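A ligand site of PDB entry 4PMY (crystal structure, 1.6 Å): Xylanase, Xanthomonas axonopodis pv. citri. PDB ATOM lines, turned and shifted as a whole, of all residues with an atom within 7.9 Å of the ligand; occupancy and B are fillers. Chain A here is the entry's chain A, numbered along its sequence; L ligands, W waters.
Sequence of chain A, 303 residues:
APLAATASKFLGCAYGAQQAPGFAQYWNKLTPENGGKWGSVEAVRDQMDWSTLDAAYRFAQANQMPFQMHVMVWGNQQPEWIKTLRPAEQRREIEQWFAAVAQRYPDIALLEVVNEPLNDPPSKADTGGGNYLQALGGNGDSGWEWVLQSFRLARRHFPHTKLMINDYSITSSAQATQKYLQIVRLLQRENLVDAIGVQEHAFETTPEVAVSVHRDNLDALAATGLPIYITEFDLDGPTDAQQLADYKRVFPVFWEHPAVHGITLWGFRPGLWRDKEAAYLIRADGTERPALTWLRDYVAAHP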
ATOM      1  N   ALA A  14      29.972 -23.552  -4.218  1.00  0.00           N
ATOM      2  CA  ALA A  14      28.891 -24.279  -4.858  1.00  0.00           C
ATOM      3  C   ALA A  14      29.284 -25.741  -5.044  1.00  0.00           C
ATOM      4  O   ALA A  14      30.411 -26.046  -5.467  1.00  0.00           O
ATOM      5  CB  ALA A  14      28.559 -23.653  -6.203  1.00  0.00           C
ATOM      6  N   GLN A  18      31.072 -31.908 -10.686  1.00  0.00           N
ATOM      7  CA  GLN A  18      32.429 -31.482 -11.050  1.00  0.00           C
ATOM      8  C   GLN A  18      33.192 -30.807  -9.910  1.00  0.00           C
ATOM      9  O   GLN A  18      34.427 -30.783  -9.923  1.00  0.00           O
ATOM     10  CB  GLN A  18      32.403 -30.579 -12.282  1.00  0.00           C
ATOM     11  CG  GLN A  18      32.031 -31.285 -13.572  1.00  0.00           C
ATOM     12  CD  GLN A  18      30.532 -31.334 -13.808  1.00  0.00           C
ATOM     13  OE1 GLN A  18      29.804 -30.432 -13.400  1.00  0.00           O
ATOM     14  NE2 GLN A  18      30.078 -32.396 -14.466  1.00  0.00           N
ATOM     15  N   PRO A  32      24.091 -26.021  -3.000  1.00  0.00           N
ATOM     16  CA  PRO A  32      23.899 -26.871  -4.178  1.00  0.00           C
ATOM     17  C   PRO A  32      23.819 -26.000  -5.430  1.00  0.00           C
ATOM     18  O   PRO A  32      23.063 -25.031  -5.456  1.00  0.00           O
ATOM     19  CB  PRO A  32      22.562 -27.574  -3.905  1.00  0.00           C
ATOM     20  CG  PRO A  32      21.851 -26.670  -2.948  1.00  0.00           C
ATOM     21  CD  PRO A  32      22.929 -26.075  -2.091  1.00  0.00           C
ATOM     22  N   GLU A  33      24.628 -26.335  -6.442  1.00  0.00           N
ATOM     23  CA  GLU A  33      24.742 -25.498  -7.631  1.00  0.00           C
ATOM     24  C   GLU A  33      23.442 -25.491  -8.443  1.00  0.00           C
ATOM     25  O   GLU A  33      22.993 -24.427  -8.889  1.00  0.00           O
ATOM     26  CB  GLU A  33      25.910 -25.972  -8.507  1.00  0.00           C
ATOM     27  CG  GLU A  33      26.230 -25.033  -9.660  1.00  0.00           C
ATOM     28  CD  GLU A  33      27.262 -25.594 -10.621  1.00  0.00           C
ATOM     29  OE1 GLU A  33      27.654 -26.771 -10.492  1.00  0.00           O
ATOM     30  OE2 GLU A  33      27.681 -24.850 -11.531  1.00  0.00           O
ATOM     31  N   ASN A  34      22.847 -26.669  -8.600  1.00  0.00           N
ATOM     32  CA  ASN A  34      21.671 -26.839  -9.472  1.00  0.00           C
ATOM     33  C   ASN A  34      20.571 -27.714  -8.881  1.00  0.00           C
ATOM     34  O   ASN A  34      19.400 -27.561  -9.225  1.00  0.00           O
ATOM     35  CB  ASN A  34      22.113 -27.408 -10.825  1.00  0.00           C
ATOM     36  CG  ASN A  34      22.742 -26.360 -11.723  1.00  0.00           C
ATOM     37  OD1 ASN A  34      22.135 -25.319 -11.990  1.00  0.00           O
ATOM     38  ND2 ASN A  34      23.958 -26.622 -12.198  1.00  0.00           N
ATOM     39  N   LYS A  37      17.190 -26.365  -7.277  1.00  0.00           N
ATOM     40  CA  LYS A  37      16.289 -25.590  -8.113  1.00  0.00           C
ATOM     41  C   LYS A  37      15.049 -26.433  -8.401  1.00  0.00           C
ATOM     42  O   LYS A  37      15.151 -27.632  -8.629  1.00  0.00           O
ATOM     43  CB  LYS A  37      16.992 -25.152  -9.392  1.00  0.00           C
ATOM     44  CG  LYS A  37      18.134 -24.175  -9.127  1.00  0.00           C
ATOM     45  CD  LYS A  37      19.058 -24.002 -10.312  1.00  0.00           C
ATOM     46  CE  LYS A  37      20.218 -23.092  -9.939  1.00  0.00           C
ATOM     47  NZ  LYS A  37      21.104 -22.807 -11.095  1.00  0.00           N
ATOM     48  N   HIS A  70      19.331 -23.529  -2.076  1.00  0.00           N
ATOM     49  CA  HIS A  70      19.340 -22.701  -3.283  1.00  0.00           C
ATOM     50  C   HIS A  70      18.537 -23.483  -4.313  1.00  0.00           C
ATOM     51  O   HIS A  70      18.993 -24.536  -4.749  1.00  0.00           O
ATOM     52  CB  HIS A  70      20.793 -22.526  -3.744  1.00  0.00           C
ATOM     53  CG  HIS A  70      20.982 -21.749  -5.012  1.00  0.00           C
ATOM     54  ND1 HIS A  70      20.896 -20.377  -5.071  1.00  0.00           N
ATOM     55  CD2 HIS A  70      21.358 -22.161  -6.254  1.00  0.00           C
ATOM     56  CE1 HIS A  70      21.166 -19.970  -6.297  1.00  0.00           C
ATOM     57  NE2 HIS A  70      21.446 -21.032  -7.037  1.00  0.00           N
ATOM     58  N   TRP A  74      12.719 -18.480  -8.238  1.00  0.00           N
ATOM     59  CA  TRP A  74      13.671 -17.931  -9.191  1.00  0.00           C
ATOM     60  C   TRP A  74      13.037 -17.950 -10.579  1.00  0.00           C
ATOM     61  O   TRP A  74      12.059 -18.654 -10.782  1.00  0.00           O
ATOM     62  CB  TRP A  74      14.959 -18.755  -9.193  1.00  0.00           C
ATOM     63  CG  TRP A  74      16.112 -18.138  -9.940  1.00  0.00           C
ATOM     64  CD1 TRP A  74      16.409 -16.814 -10.034  1.00  0.00           C
ATOM     65  CD2 TRP A  74      17.130 -18.833 -10.657  1.00  0.00           C
ATOM     66  NE1 TRP A  74      17.549 -16.637 -10.778  1.00  0.00           N
ATOM     67  CE2 TRP A  74      18.011 -17.864 -11.182  1.00  0.00           C
ATOM     68  CE3 TRP A  74      17.380 -20.184 -10.924  1.00  0.00           C
ATOM     69  CZ2 TRP A  74      19.137 -18.197 -11.945  1.00  0.00           C
ATOM     70  CZ3 TRP A  74      18.498 -20.516 -11.694  1.00  0.00           C
ATOM     71  CH2 TRP A  74      19.357 -19.526 -12.190  1.00  0.00           C
ATOM     72  N   ASN A  76      14.426 -18.817 -13.590  1.00  0.00           N
ATOM     73  CA  ASN A  76      14.886 -19.824 -14.546  1.00  0.00           C
ATOM     74  C   ASN A  76      15.060 -21.183 -13.866  1.00  0.00           C
ATOM     75  O   ASN A  76      15.006 -21.280 -12.634  1.00  0.00           O
ATOM     76  CB  ASN A  76      16.172 -19.379 -15.270  1.00  0.00           C
ATOM     77  CG  ASN A  76      16.157 -19.726 -16.756  1.00  0.00           C
ATOM     78  OD1 ASN A  76      16.825 -19.071 -17.566  1.00  0.00           O
ATOM     79  ND2 ASN A  76      15.398 -20.744 -17.132  1.00  0.00           N
ATOM     80  N   GLN A  77      15.248 -22.236 -14.667  1.00  0.00           N
ATOM     81  CA  GLN A  77      15.327 -23.611 -14.155  1.00  0.00           C
ATOM     82  C   GLN A  77      14.157 -23.951 -13.230  1.00  0.00           C
ATOM     83  O   GLN A  77      14.334 -24.622 -12.202  1.00  0.00           O
ATOM     84  CB  GLN A  77      16.690 -23.871 -13.480  1.00  0.00           C
ATOM     85  CG  GLN A  77      17.830 -23.978 -14.492  1.00  0.00           C
ATOM     86  CD  GLN A  77      19.182 -24.009 -13.834  1.00  0.00           C
ATOM     87  OE1 GLN A  77      19.754 -22.972 -13.516  1.00  0.00           O
ATOM     88  NE2 GLN A  77      19.717 -25.205 -13.628  1.00  0.00           N
ATOM     89  N   ASN A 115      15.757 -15.631  -5.409  1.00  0.00           N
ATOM     90  CA  ASN A 115      16.977 -15.208  -6.089  1.00  0.00           C
ATOM     91  C   ASN A 115      16.652 -14.266  -7.232  1.00  0.00           C
ATOM     92  O   ASN A 115      15.675 -14.470  -7.971  1.00  0.00           O
ATOM     93  CB  ASN A 115      17.749 -16.429  -6.607  1.00  0.00           C
ATOM     94  CG  ASN A 115      19.131 -16.083  -7.132  1.00  0.00           C
ATOM     95  OD1 ASN A 115      19.774 -15.146  -6.664  1.00  0.00           O
ATOM     96  ND2 ASN A 115      19.596 -16.848  -8.108  1.00  0.00           N
ATOM     97  N   GLU A 116      17.471 -13.219  -7.384  1.00  0.00           N
ATOM     98  CA  GLU A 116      17.433 -12.289  -8.522  1.00  0.00           C
ATOM     99  C   GLU A 116      16.117 -11.527  -8.773  1.00  0.00           C
ATOM    100  O   GLU A 116      15.657 -11.453  -9.919  1.00  0.00           O
ATOM    101  CB  GLU A 116      17.939 -12.973  -9.797  1.00  0.00           C
ATOM    102  CG  GLU A 116      19.382 -13.442  -9.701  1.00  0.00           C
ATOM    103  CD  GLU A 116      19.821 -14.326 -10.847  1.00  0.00           C
ATOM    104  OE1 GLU A 116      19.063 -14.482 -11.833  1.00  0.00           O
ATOM    105  OE2 GLU A 116      20.934 -14.879 -10.781  1.00  0.00           O
ATOM    106  N   GLN A 199      25.559 -11.774  -5.057  1.00  0.00           N
ATOM    107  CA  GLN A 199      26.308 -12.822  -5.754  1.00  0.00           C
ATOM    108  C   GLN A 199      27.799 -12.515  -5.951  1.00  0.00           C
ATOM    109  O   GLN A 199      28.652 -13.320  -5.570  1.00  0.00           O
ATOM    110  CB  GLN A 199      25.618 -13.186  -7.077  1.00  0.00           C
ATOM    111  CG  GLN A 199      24.265 -13.868  -6.873  1.00  0.00           C
ATOM    112  CD  GLN A 199      23.590 -14.233  -8.183  1.00  0.00           C
ATOM    113  OE1 GLN A 199      24.228 -14.288  -9.235  1.00  0.00           O
ATOM    114  NE2 GLN A 199      22.287 -14.493  -8.120  1.00  0.00           N
ATOM    115  N   HIS A 201      29.531 -12.199  -8.912  1.00  0.00           N
ATOM    116  CA  HIS A 201      30.187 -12.859 -10.035  1.00  0.00           C
ATOM    117  C   HIS A 201      31.183 -11.904 -10.694  1.00  0.00           C
ATOM    118  O   HIS A 201      31.139 -10.694 -10.454  1.00  0.00           O
ATOM    119  CB  HIS A 201      29.166 -13.326 -11.079  1.00  0.00           C
ATOM    120  CG  HIS A 201      28.333 -14.490 -10.636  1.00  0.00           C
ATOM    121  ND1 HIS A 201      28.805 -15.787 -10.631  1.00  0.00           N
ATOM    122  CD2 HIS A 201      27.063 -14.550 -10.187  1.00  0.00           C
ATOM    123  CE1 HIS A 201      27.863 -16.598 -10.199  1.00  0.00           C
ATOM    124  NE2 HIS A 201      26.786 -15.870  -9.916  1.00  0.00           N
ATOM    125  N   GLU A 232      27.862 -16.016  -4.579  1.00  0.00           N
ATOM    126  CA  GLU A 232      28.244 -16.683  -5.830  1.00  0.00           C
ATOM    127  C   GLU A 232      29.481 -16.031  -6.455  1.00  0.00           C
ATOM    128  O   GLU A 232      29.466 -15.590  -7.608  1.00  0.00           O
ATOM    129  CB  GLU A 232      27.054 -16.725  -6.792  1.00  0.00           C
ATOM    130  CG  GLU A 232      25.788 -17.264  -6.149  1.00  0.00           C
ATOM    131  CD  GLU A 232      24.599 -17.379  -7.076  1.00  0.00           C
ATOM    132  OE1 GLU A 232      24.773 -17.266  -8.307  1.00  0.00           O
ATOM    133  OE2 GLU A 232      23.487 -17.594  -6.554  1.00  0.00           O
ATOM    134  N   ASP A 234      32.949 -15.305  -8.118  1.00  0.00           N
ATOM    135  CA  ASP A 234      33.916 -15.835  -9.077  1.00  0.00           C
ATOM    136  C   ASP A 234      34.658 -14.716  -9.789  1.00  0.00           C
ATOM    137  O   ASP A 234      34.171 -13.577  -9.843  1.00  0.00           O
ATOM    138  CB  ASP A 234      33.287 -16.855 -10.063  1.00  0.00           C
ATOM    139  CG  ASP A 234      32.069 -16.319 -10.794  1.00  0.00           C
ATOM    140  OD1 ASP A 234      32.064 -15.151 -11.234  1.00  0.00           O
ATOM    141  OD2 ASP A 234      31.102 -17.083 -10.972  1.00  0.00           O
ATOM    142  N   TRP A 266      31.463 -19.457  -6.420  1.00  0.00           N
ATOM    143  CA  TRP A 266      30.623 -20.197  -7.340  1.00  0.00           C
ATOM    144  C   TRP A 266      31.399 -21.214  -8.172  1.00  0.00           C
ATOM    145  O   TRP A 266      31.490 -21.097  -9.399  1.00  0.00           O
ATOM    146  CB  TRP A 266      29.757 -19.278  -8.214  1.00  0.00           C
ATOM    147  CG  TRP A 266      28.516 -20.003  -8.637  1.00  0.00           C
ATOM    148  CD1 TRP A 266      28.192 -20.408  -9.897  1.00  0.00           C
ATOM    149  CD2 TRP A 266      27.477 -20.485  -7.775  1.00  0.00           C
ATOM    150  NE1 TRP A 266      26.988 -21.080  -9.882  1.00  0.00           N
ATOM    151  CE2 TRP A 266      26.539 -21.145  -8.588  1.00  0.00           C
ATOM    152  CE3 TRP A 266      27.260 -20.404  -6.393  1.00  0.00           C
ATOM    153  CZ2 TRP A 266      25.380 -21.735  -8.060  1.00  0.00           C
ATOM    154  CZ3 TRP A 266      26.106 -20.986  -5.870  1.00  0.00           C
ATOM    155  CH2 TRP A 266      25.175 -21.638  -6.705  1.00  0.00           C
ATOM    156  N   GLY A 267      31.946 -22.224  -7.496  1.00  0.00           N
ATOM    157  CA  GLY A 267      32.747 -23.266  -8.129  1.00  0.00           C
ATOM    158  C   GLY A 267      34.232 -22.971  -8.013  1.00  0.00           C
ATOM    159  O   GLY A 267      34.634 -21.827  -7.791  1.00  0.00           O
ATOM    160  N   GLY A 271      34.349 -26.783 -15.174  1.00  0.00           N
ATOM    161  CA  GLY A 271      32.971 -27.260 -15.207  1.00  0.00           C
ATOM    162  C   GLY A 271      32.052 -26.411 -14.339  1.00  0.00           C
ATOM    163  O   GLY A 271      30.843 -26.644 -14.305  1.00  0.00           O
ATOM    164  N   LEU A 272      32.634 -25.435 -13.641  1.00  0.00           N
ATOM    165  CA  LEU A 272      31.862 -24.408 -12.935  1.00  0.00           C
ATOM    166  C   LEU A 272      31.140 -23.525 -13.949  1.00  0.00           C
ATOM    167  O   LEU A 272      31.387 -23.637 -15.156  1.00  0.00           O
ATOM    168  CB  LEU A 272      32.777 -23.578 -12.012  1.00  0.00           C
ATOM    169  CG  LEU A 272      33.613 -22.405 -12.565  1.00  0.00           C
ATOM    170  CD1 LEU A 272      34.386 -21.766 -11.427  1.00  0.00           C
ATOM    171  CD2 LEU A 272      34.555 -22.829 -13.681  1.00  0.00           C
ATOM    172  N   TRP A 273      30.249 -22.651 -13.478  1.00  0.00           N
ATOM    173  CA  TRP A 273      29.409 -21.865 -14.383  1.00  0.00           C
ATOM    174  C   TRP A 273      30.219 -21.083 -15.419  1.00  0.00           C
ATOM    175  O   TRP A 273      29.986 -21.198 -16.622  1.00  0.00           O
ATOM    176  CB  TRP A 273      28.469 -20.937 -13.604  1.00  0.00           C
ATOM    177  CG  TRP A 273      27.589 -20.095 -14.485  1.00  0.00           C
ATOM    178  CD1 TRP A 273      26.779 -20.531 -15.494  1.00  0.00           C
ATOM    179  CD2 TRP A 273      27.420 -18.674 -14.426  1.00  0.00           C
ATOM    180  NE1 TRP A 273      26.126 -19.469 -16.072  1.00  0.00           N
ATOM    181  CE2 TRP A 273      26.499 -18.324 -15.433  1.00  0.00           C
ATOM    182  CE3 TRP A 273      27.959 -17.664 -13.613  1.00  0.00           C
ATOM    183  CZ2 TRP A 273      26.108 -16.996 -15.666  1.00  0.00           C
ATOM    184  CZ3 TRP A 273      27.575 -16.351 -13.841  1.00  0.00           C
ATOM    185  CH2 TRP A 273      26.656 -16.028 -14.868  1.00  0.00           C
ATOM    186  N   ARG A 274      31.198 -20.318 -14.931  1.00  0.00           N
ATOM    187  CA  ARG A 274      32.028 -19.507 -15.817  1.00  0.00           C
ATOM    188  C   ARG A 274      33.266 -20.274 -16.291  1.00  0.00           C
ATOM    189  O   ARG A 274      34.401 -19.827 -16.133  1.00  0.00           O
ATOM    190  CB  ARG A 274      32.398 -18.181 -15.135  1.00  0.00           C
ATOM    191  CG  ARG A 274      31.183 -17.313 -14.842  1.00  0.00           C
ATOM    192  CD  ARG A 274      31.535 -15.947 -14.287  1.00  0.00           C
ATOM    193  NE  ARG A 274      32.176 -15.071 -15.268  1.00  0.00           N
ATOM    194  CZ  ARG A 274      31.533 -14.375 -16.213  1.00  0.00           C
ATOM    195  NH1 ARG A 274      30.215 -14.462 -16.342  1.00  0.00           N
ATOM    196  NH2 ARG A 274      32.229 -13.599 -17.040  1.00  0.00           N
HETATM  197  O1  LIG L   1      24.303 -20.841 -11.117  1.00  0.00           O
HETATM  198  C1  LIG L   1      24.234 -21.261 -12.475  1.00  0.00           C
HETATM  199  C2  LIG L   1      24.757 -22.684 -12.591  1.00  0.00           C
HETATM  200  C3  LIG L   1      24.609 -23.195 -14.022  1.00  0.00           C
HETATM  201  C4  LIG L   1      23.182 -22.968 -14.520  1.00  0.00           C
HETATM  202  C5  LIG L   1      22.732 -21.528 -14.302  1.00  0.00           C
HETATM  203  O2  LIG L   1      26.144 -22.735 -12.222  1.00  0.00           O
HETATM  204  O3  LIG L   1      24.933 -24.596 -14.058  1.00  0.00           O
HETATM  205  O4  LIG L   1      23.125 -23.280 -15.908  1.00  0.00           O
HETATM  206  O5  LIG L   1      22.881 -21.177 -12.924  1.00  0.00           O
HETATM  207  O   HOH W   1      28.115 -25.653 -14.103  1.00  0.00           O
HETATM  208  O   HOH W   2      22.139 -20.462  -9.668  1.00  0.00           O
HETATM  209  O   HOH W   3      25.183 -18.485 -10.660  1.00  0.00           O
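Trp 74 touches the ligand.
OE1 of Gln 77 touches C5 of the ligand, at 3.4 Å.
Trp 273 touches the ligand (CB to O2, 3.2 Å).
Hydrophobic or aromatic side chains within 4 Å of the ligand: Trp 74, Trp 266 and Trp 273.
Seven residues have an atom within 4 Å of the ligand: Glu 33, Asn 34, Lys 37, Trp 74, Gln 77, Trp 266 and Trp 273.
The nearest printed residue that does not touch the ligand is Glu 232 (4.6 Å).
Water W3 lies within hydrogen-bond range of an oxygen (O1) of the ligand (2.6 Å), the side-chain carboxylate (OE1) of Glu 232 (2.7 Å), a ring nitrogen (NE2) of His 201 (3.2 Å) and the indole nitrogen (NE1) of Trp 266 (3.3 Å).
Water W2 lies within hydrogen-bond range of O1 of the ligand (2.6 Å), NE2 of His 70 (2.8 Å) and NZ of Lys 37 (2.9 Å).
Water W1 lies within hydrogen-bond range of OE2 of Glu 33 (2.7 Å), O of Gly 271 (2.9 Å) and O3 of the ligand (3.4 Å).
An oxygen (O5) of the ligand lies within hydrogen-bond range of the side-chain amino group (NZ) of Lys 37, 3.0 Å away.
An oxygen (O3) of the ligand is in hydrogen-bond range of the side-chain amide nitrogen (ND2) of Asn 34 (2.9 Å).
The indole nitrogen (NE1) of Trp 266 lies within hydrogen-bond range of an oxygen (O1) of the ligand.
The side-chain carboxylate of Glu 33 sits at hydrogen-bond distance from an oxygen (O2) of the ligand.
NE2 of Gln 77 is in hydrogen-bond range of OD1 of Asn 34 (2.9 Å).
The side-chain amide oxygen (OD1) of Asn 34 lies within hydrogen-bond range of the side-chain amino group (NZ) of Lys 37 (2.9 Å).
The side-chain amino group (NZ) of Lys 37 lies close to the backbone carbonyl oxygen (O) of Glu 33, at 3.3 Å.
The indole nitrogen (NE1) of Trp 74 is in hydrogen-bond range of the side-chain carboxylate (OE1) of Glu 116 (2.8 Å).
NE1 of Trp 74 sits close to ND2 of Asn 115, at 3.4 Å.
The side-chain amino group (NZ) of Lys 37 sits at hydrogen-bond distance from the side-chain amide oxygen (OE1) of Gln 77, 2.8 Å away.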
